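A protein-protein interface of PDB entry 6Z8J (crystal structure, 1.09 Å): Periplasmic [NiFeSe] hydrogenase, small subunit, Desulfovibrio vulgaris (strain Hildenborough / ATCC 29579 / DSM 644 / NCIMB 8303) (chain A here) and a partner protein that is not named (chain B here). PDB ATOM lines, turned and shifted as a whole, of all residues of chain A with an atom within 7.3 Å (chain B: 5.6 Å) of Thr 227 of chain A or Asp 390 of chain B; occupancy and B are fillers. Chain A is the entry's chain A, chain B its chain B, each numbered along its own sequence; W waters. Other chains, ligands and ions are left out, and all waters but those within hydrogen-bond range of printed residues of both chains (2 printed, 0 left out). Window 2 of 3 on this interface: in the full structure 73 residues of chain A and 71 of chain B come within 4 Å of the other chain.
OD1 of Asp 390 of chain B is in hydrogen-bond range of N of Val 392 of chain B, 3.3 Å away. O of Lys 229 of chain A lies within hydrogen-bond range of NH1 of Arg 233 of chain A. The side-chain hydroxyl of Thr 227 of chain A lies within hydrogen-bond range of the side-chain hydroxyl of Thr 225 of chain A, 3.4 Å away. NZ of Lys 229 of chain A lies within hydrogen-bond range of O of Phe 226 of chain A (2.8 Å). The backbone carbonyl oxygen of Asn 262 of chain A sits at hydrogen-bond distance from the side-chain amino group of Lys 229 of chain A, 2.8 Å away. O of Ala 183 of chain B sits at hydrogen-bond distance from OG1 of Thr 391 of chain B (2.8 Å).
The side-chain carboxylate (OD1) of Asp 390 of chain B lies within hydrogen-bond range of the side-chain hydroxyl (OG1) of Thr 227 of chain A (2.9 Å). The side-chain carboxylate of Glu 185 of chain B lies within hydrogen-bond range of the side-chain amide nitrogen of Asn 262 of chain A (2.9 Å). NZ of Lys 229 of chain A lies within hydrogen-bond range of O of Thr 184 of chain B (3.0 Å). The backbone carbonyl oxygen (O) of Phe 226 of chain A sits close to the backbone carbonyl oxygen (O) of Thr 184 of chain B. O of Asn 262 of chain A is in hydrogen-bond range of OG1 of Thr 184 of chain B, at 2.8 Å.
Water W2 lies within hydrogen-bond range of O of Thr 227 of chain A (2.7 Å) and N of Ile 186 of chain B (2.9 Å). Water W1 lies within hydrogen-bond range of OG1 of Thr 225 of chain A (2.8 Å), O of Val 392 of chain B (2.9 Å) and OD2 of Asp 390 of chain B (2.9 Å).
Thr 227 of chain A touches just these residues of chain B: Ala 183, Thr 184, Ile 186, Asp 390, Thr 391 and Val 392. Asp 228 of chain A touches none of the printed residues of chain B. Gly 91 of chain B touches none of the printed residues of chain A. Of the printed residues of chain A, Thr 184 of chain B touches Phe 226, Thr 227, Lys 229 and Asn 262. Of the printed residues of chain A, Glu 185 of chain B touches Asn 262. Of the printed residues of chain A, Ile 186 of chain B touches Thr 227 (3.8 Å). Of chain A, only Thr 227 comes within 4 Å of Asp 390 of chain B. Printed residues of chain A within 4 Å of Thr 391 of chain B: Thr 227. Of the printed residues of chain A, Val 392 of chain B touches Thr 225 (3.2 Å) and Thr 227 (3.7 Å). The nearest printed residue of chain B that does not touch Asn 262 of chain A is Ala 183 of chain B (6.4 Å).
Of the 11 printed residues of chain A, 5 touch a printed residue of chain B. Hydrophobic or aromatic side chains of chain A that line the printed part of chain B: Phe 226. Of the 13 printed residues of chain B, 7 touch a printed residue of chain A. Hydrophobic or aromatic side chains of chain B within 4 Å of the printed part of chain A: Ile 186 and Val 392. Among the printed residues, 11 pairs touch across the chains.
Among the printed residues, pairs that only touch across the chains: Thr 225 of chain A with Val 392 of chain B, Thr 227 of chain A with Ala 183 of chain B, Thr 227 of chain A with Thr 184 of chain B, Thr 227 of chain A with Ile 186 of chain B, Thr 227 of chain A with Thr 391 of chain B and Thr 227 of chain A with Val 392 of chain B.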
ATOM      1  N   SER A 223     -15.509   9.663  10.134  1.00  0.00           N
ATOM      2  CA  SER A 223     -16.677  10.522  10.226  1.00  0.00           C
ATOM      3  C   SER A 223     -17.963   9.700  10.187  1.00  0.00           C
ATOM      4  O   SER A 223     -18.096   8.740   9.416  1.00  0.00           O
ATOM      5  CB  SER A 223     -16.657  11.559   9.107  1.00  0.00           C
ATOM      6  OG  SER A 223     -15.553  12.425   9.309  1.00  0.00           O
ATOM      7  N   ALA A 224     -18.922  10.095  11.023  1.00  0.00           N
ATOM      8  CA  ALA A 224     -20.242   9.477  11.078  1.00  0.00           C
ATOM      9  C   ALA A 224     -21.300  10.297  10.363  1.00  0.00           C
ATOM     10  O   ALA A 224     -22.399   9.789  10.124  1.00  0.00           O
ATOM     11  CB  ALA A 224     -20.665   9.293  12.540  1.00  0.00           C
ATOM     12  N   THR A 225     -21.001  11.557  10.059  1.00  0.00           N
ATOM     13  CA  THR A 225     -21.849  12.398   9.236  1.00  0.00           C
ATOM     14  C   THR A 225     -21.011  13.000   8.116  1.00  0.00           C
ATOM     15  O   THR A 225     -19.816  13.265   8.282  1.00  0.00           O
ATOM     16  CB  THR A 225     -22.540  13.519  10.037  1.00  0.00           C
ATOM     17  OG1 THR A 225     -23.227  14.349   9.094  1.00  0.00           O
ATOM     18  CG2 THR A 225     -21.544  14.371  10.867  1.00  0.00           C
ATOM     19  N   PHE A 226     -21.638  13.216   6.962  1.00  0.00           N
ATOM     20  CA  PHE A 226     -20.880  13.712   5.825  1.00  0.00           C
ATOM     21  C   PHE A 226     -20.223  15.046   6.125  1.00  0.00           C
ATOM     22  O   PHE A 226     -19.149  15.330   5.590  1.00  0.00           O
ATOM     23  CB  PHE A 226     -21.767  13.921   4.601  1.00  0.00           C
ATOM     24  CG  PHE A 226     -22.299  12.664   4.006  1.00  0.00           C
ATOM     25  CD1 PHE A 226     -21.465  11.795   3.308  1.00  0.00           C
ATOM     26  CD2 PHE A 226     -23.649  12.361   4.106  1.00  0.00           C
ATOM     27  CE1 PHE A 226     -21.973  10.639   2.741  1.00  0.00           C
ATOM     28  CE2 PHE A 226     -24.163  11.212   3.546  1.00  0.00           C
ATOM     29  CZ  PHE A 226     -23.325  10.351   2.859  1.00  0.00           C
ATOM     30  N   THR A 227     -20.852  15.885   6.955  1.00  0.00           N
ATOM     31  CA  THR A 227     -20.346  17.241   7.146  1.00  0.00           C
ATOM     32  C   THR A 227     -19.174  17.316   8.114  1.00  0.00           C
ATOM     33  O   THR A 227     -18.585  18.395   8.267  1.00  0.00           O
ATOM     34  CB  THR A 227     -21.473  18.160   7.615  1.00  0.00           C
ATOM     35  OG1 THR A 227     -22.126  17.539   8.723  1.00  0.00           O
ATOM     36  CG2 THR A 227     -22.467  18.396   6.485  1.00  0.00           C
ATOM     37  N   ASP A 228     -18.808  16.207   8.751  1.00  0.00           N
ATOM     38  CA  ASP A 228     -17.608  16.143   9.575  1.00  0.00           C
ATOM     39  C   ASP A 228     -16.432  15.878   8.651  1.00  0.00           C
ATOM     40  O   ASP A 228     -16.270  14.759   8.144  1.00  0.00           O
ATOM     41  CB  ASP A 228     -17.757  15.016  10.588  1.00  0.00           C
ATOM     42  CG  ASP A 228     -16.532  14.831  11.449  1.00  0.00           C
ATOM     43  OD1 ASP A 228     -15.504  15.491  11.197  1.00  0.00           O
ATOM     44  OD2 ASP A 228     -16.604  14.012  12.385  1.00  0.00           O
ATOM     45  N   LYS A 229     -15.622  16.899   8.414  1.00  0.00           N
ATOM     46  CA  LYS A 229     -14.507  16.796   7.482  1.00  0.00           C
ATOM     47  C   LYS A 229     -13.198  16.384   8.149  1.00  0.00           C
ATOM     48  O   LYS A 229     -12.170  16.320   7.467  1.00  0.00           O
ATOM     49  CB  LYS A 229     -14.339  18.127   6.749  1.00  0.00           C
ATOM     50  CG  LYS A 229     -15.589  18.582   5.978  1.00  0.00           C
ATOM     51  CD  LYS A 229     -16.201  17.440   5.144  1.00  0.00           C
ATOM     52  CE  LYS A 229     -17.236  17.929   4.179  1.00  0.00           C
ATOM     53  NZ  LYS A 229     -17.849  16.758   3.509  1.00  0.00           N
ATOM     54  N   VAL A 230     -13.216  16.086   9.449  1.00  0.00           N
ATOM     55  CA  VAL A 230     -12.008  15.660  10.154  1.00  0.00           C
ATOM     56  C   VAL A 230     -11.677  14.202   9.858  1.00  0.00           C
ATOM     57  O   VAL A 230     -10.523  13.853   9.600  1.00  0.00           O
ATOM     58  CB  VAL A 230     -12.159  15.896  11.671  1.00  0.00           C
ATOM     59  CG1 VAL A 230     -11.018  15.206  12.459  1.00  0.00           C
ATOM     60  CG2 VAL A 230     -12.188  17.392  11.970  1.00  0.00           C
ATOM     61  N   ARG A 233     -13.536   8.990   5.451  1.00  0.00           N
ATOM     62  CA  ARG A 233     -14.865   8.805   4.876  1.00  0.00           C
ATOM     63  C   ARG A 233     -15.184   7.341   4.585  1.00  0.00           C
ATOM     64  O   ARG A 233     -16.223   7.055   3.984  1.00  0.00           O
ATOM     65  CB  ARG A 233     -14.988   9.616   3.580  1.00  0.00           C
ATOM     66  CG  ARG A 233     -15.069  11.129   3.741  1.00  0.00           C
ATOM     67  CD  ARG A 233     -13.844  11.825   4.270  1.00  0.00           C
ATOM     68  NE  ARG A 233     -13.886  13.225   3.849  1.00  0.00           N
ATOM     69  CZ  ARG A 233     -13.335  14.253   4.490  1.00  0.00           C
ATOM     70  NH1 ARG A 233     -12.676  14.083   5.628  1.00  0.00           N
ATOM     71  NH2 ARG A 233     -13.468  15.476   3.987  1.00  0.00           N
ATOM     72  N   LEU A 236     -18.566   6.001   5.623  1.00  0.00           N
ATOM     73  CA  LEU A 236     -19.620   6.662   4.870  1.00  0.00           C
ATOM     74  C   LEU A 236     -19.708   6.138   3.441  1.00  0.00           C
ATOM     75  O   LEU A 236     -20.580   6.574   2.695  1.00  0.00           O
ATOM     76  CB  LEU A 236     -19.364   8.176   4.859  1.00  0.00           C
ATOM     77  CG  LEU A 236     -19.499   8.920   6.194  1.00  0.00           C
ATOM     78  CD1 LEU A 236     -18.913  10.315   6.084  1.00  0.00           C
ATOM     79  CD2 LEU A 236     -20.958   8.980   6.653  1.00  0.00           C
ATOM     80  N   ASN A 262     -15.601  16.620  -0.325  1.00  0.00           N
ATOM     81  CA  ASN A 262     -17.002  17.046  -0.289  1.00  0.00           C
ATOM     82  C   ASN A 262     -17.936  15.985   0.285  1.00  0.00           C
ATOM     83  O   ASN A 262     -18.902  16.315   0.988  1.00  0.00           O
ATOM     84  CB  ASN A 262     -17.414  17.370  -1.726  1.00  0.00           C
ATOM     85  CG  ASN A 262     -18.867  17.732  -1.872  1.00  0.00           C
ATOM     86  OD1 ASN A 262     -19.630  17.007  -2.508  1.00  0.00           O
ATOM     87  ND2 ASN A 262     -19.257  18.878  -1.319  1.00  0.00           N
ATOM     88  N   PRO B  88     -31.895  20.284   7.329  1.00  0.00           N
ATOM     89  CA  PRO B  88     -31.657  21.508   8.091  1.00  0.00           C
ATOM     90  C   PRO B  88     -31.790  22.726   7.197  1.00  0.00           C
ATOM     91  O   PRO B  88     -31.450  22.695   6.011  1.00  0.00           O
ATOM     92  CB  PRO B  88     -30.213  21.355   8.580  1.00  0.00           C
ATOM     93  CG  PRO B  88     -29.970  19.878   8.567  1.00  0.00           C
ATOM     94  CD  PRO B  88     -30.784  19.326   7.442  1.00  0.00           C
ATOM     95  N   ASN B  89     -32.233  23.827   7.803  1.00  0.00           N
ATOM     96  CA  ASN B  89     -32.404  25.077   7.065  1.00  0.00           C
ATOM     97  C   ASN B  89     -31.169  25.423   6.232  1.00  0.00           C
ATOM     98  O   ASN B  89     -31.280  25.768   5.051  1.00  0.00           O
ATOM     99  CB  ASN B  89     -32.706  26.200   8.053  1.00  0.00           C
ATOM    100  CG  ASN B  89     -32.959  27.511   7.375  1.00  0.00           C
ATOM    101  OD1 ASN B  89     -33.965  27.678   6.711  1.00  0.00           O
ATOM    102  ND2 ASN B  89     -32.058  28.456   7.549  1.00  0.00           N
ATOM    103  N   ASN B  90     -29.971  25.315   6.814  1.00  0.00           N
ATOM    104  CA  ASN B  90     -28.775  25.729   6.084  1.00  0.00           C
ATOM    105  C   ASN B  90     -28.473  24.782   4.930  1.00  0.00           C
ATOM    106  O   ASN B  90     -27.871  25.190   3.932  1.00  0.00           O
ATOM    107  CB  ASN B  90     -27.572  25.846   7.032  1.00  0.00           C
ATOM    108  CG  ASN B  90     -26.621  26.941   6.619  1.00  0.00           C
ATOM    109  OD1 ASN B  90     -27.035  28.049   6.293  1.00  0.00           O
ATOM    110  ND2 ASN B  90     -25.339  26.630   6.612  1.00  0.00           N
ATOM    111  N   GLY B  91     -28.878  23.519   5.051  1.00  0.00           N
ATOM    112  CA  GLY B  91     -28.727  22.589   3.945  1.00  0.00           C
ATOM    113  C   GLY B  91     -29.699  22.849   2.805  1.00  0.00           C
ATOM    114  O   GLY B  91     -29.360  22.650   1.638  1.00  0.00           O
ATOM    115  N   ALA B 183     -27.169  18.476   2.460  1.00  0.00           N
ATOM    116  CA  ALA B 183     -25.979  18.718   1.663  1.00  0.00           C
ATOM    117  C   ALA B 183     -24.764  18.291   2.475  1.00  0.00           C
ATOM    118  O   ALA B 183     -24.726  18.487   3.693  1.00  0.00           O
ATOM    119  CB  ALA B 183     -25.880  20.193   1.295  1.00  0.00           C
ATOM    120  N   THR B 184     -23.783  17.692   1.810  1.00  0.00           N
ATOM    121  CA  THR B 184     -22.703  16.978   2.488  1.00  0.00           C
ATOM    122  C   THR B 184     -21.582  17.877   3.009  1.00  0.00           C
ATOM    123  O   THR B 184     -20.726  17.384   3.754  1.00  0.00           O
ATOM    124  CB  THR B 184     -22.060  15.984   1.525  1.00  0.00           C
ATOM    125  OG1 THR B 184     -21.563  16.706   0.398  1.00  0.00           O
ATOM    126  CG2 THR B 184     -23.032  14.921   1.042  1.00  0.00           C
ATOM    127  N   GLU B 185     -21.553  19.152   2.629  1.00  0.00           N
ATOM    128  CA  GLU B 185     -20.467  20.059   2.978  1.00  0.00           C
ATOM    129  C   GLU B 185     -21.048  21.383   3.457  1.00  0.00           C
ATOM    130  O   GLU B 185     -21.697  22.104   2.689  1.00  0.00           O
ATOM    131  CB  GLU B 185     -19.518  20.277   1.800  1.00  0.00           C
ATOM    132  CG  GLU B 185     -18.437  21.265   2.137  1.00  0.00           C
ATOM    133  CD  GLU B 185     -17.387  21.399   1.071  1.00  0.00           C
ATOM    134  OE1 GLU B 185     -17.421  20.650   0.081  1.00  0.00           O
ATOM    135  OE2 GLU B 185     -16.517  22.281   1.234  1.00  0.00           O
ATOM    136  N   ILE B 186     -20.807  21.696   4.718  1.00  0.00           N
ATOM    137  CA  ILE B 186     -21.200  22.990   5.284  1.00  0.00           C
ATOM    138  C   ILE B 186     -20.409  24.099   4.597  1.00  0.00           C
ATOM    139  O   ILE B 186     -19.171  24.042   4.574  1.00  0.00           O
ATOM    140  CB  ILE B 186     -20.926  23.000   6.788  1.00  0.00           C
ATOM    141  CG1 ILE B 186     -21.808  21.978   7.509  1.00  0.00           C
ATOM    142  CG2 ILE B 186     -21.142  24.404   7.353  1.00  0.00           C
ATOM    143  CD1 ILE B 186     -21.405  21.760   8.936  1.00  0.00           C
ATOM    144  N   GLY B 388     -20.793  27.724   8.550  1.00  0.00           N
ATOM    145  CA  GLY B 388     -20.617  26.838   9.678  1.00  0.00           C
ATOM    146  C   GLY B 388     -21.848  26.117  10.194  1.00  0.00           C
ATOM    147  O   GLY B 388     -21.699  25.198  11.007  1.00  0.00           O
ATOM    148  N   GLU B 389     -23.057  26.482   9.765  1.00  0.00           N
ATOM    149  CA  GLU B 389     -24.254  25.829  10.300  1.00  0.00           C
ATOM    150  C   GLU B 389     -24.526  24.510   9.580  1.00  0.00           C
ATOM    151  O   GLU B 389     -24.376  24.417   8.359  1.00  0.00           O
ATOM    152  CB  GLU B 389     -25.475  26.750  10.198  1.00  0.00           C
ATOM    153  CG  GLU B 389     -25.434  27.956  11.131  1.00  0.00           C
ATOM    154  CD  GLU B 389     -26.738  28.738  11.164  1.00  0.00           C
ATOM    155  OE1 GLU B 389     -27.735  28.298  10.539  1.00  0.00           O
ATOM    156  OE2 GLU B 389     -26.752  29.805  11.817  1.00  0.00           O
ATOM    157  N   ASP B 390     -24.936  23.483  10.343  1.00  0.00           N
ATOM    158  CA  ASP B 390     -25.014  22.143   9.764  1.00  0.00           C
ATOM    159  C   ASP B 390     -26.003  22.098   8.606  1.00  0.00           C
ATOM    160  O   ASP B 390     -27.009  22.821   8.561  1.00  0.00           O
ATOM    161  CB  ASP B 390     -25.348  21.052  10.788  1.00  0.00           C
ATOM    162  CG  ASP B 390     -24.701  19.658  10.426  1.00  0.00           C
ATOM    163  OD1 ASP B 390     -24.398  19.332   9.226  1.00  0.00           O
ATOM    164  OD2 ASP B 390     -24.505  18.874  11.387  1.00  0.00           O
ATOM    165  N   THR B 391     -25.685  21.242   7.654  1.00  0.00           N
ATOM    166  CA  THR B 391     -26.437  21.142   6.423  1.00  0.00           C
ATOM    167  C   THR B 391     -27.010  19.758   6.177  1.00  0.00           C
ATOM    168  O   THR B 391     -27.685  19.569   5.166  1.00  0.00           O
ATOM    169  CB  THR B 391     -25.538  21.509   5.240  1.00  0.00           C
ATOM    170  OG1 THR B 391     -24.331  20.745   5.319  1.00  0.00           O
ATOM    171  CG2 THR B 391     -25.211  22.996   5.245  1.00  0.00           C
ATOM    172  N   VAL B 392     -26.758  18.780   7.041  1.00  0.00           N
ATOM    173  CA  VAL B 392     -27.201  17.418   6.764  1.00  0.00           C
ATOM    174  C   VAL B 392     -27.641  16.710   8.035  1.00  0.00           C
ATOM    175  O   VAL B 392     -27.131  16.976   9.127  1.00  0.00           O
ATOM    176  CB  VAL B 392     -26.086  16.621   6.033  1.00  0.00           C
ATOM    177  CG1 VAL B 392     -25.134  15.950   7.028  1.00  0.00           C
ATOM    178  CG2 VAL B 392     -26.690  15.603   5.065  1.00  0.00           C
HETATM  179  O   HOH W   1     -24.849  16.091  10.609  1.00  0.00           O
HETATM  180  O   HOH W   2     -18.856  20.181   6.200  1.00  0.00           O
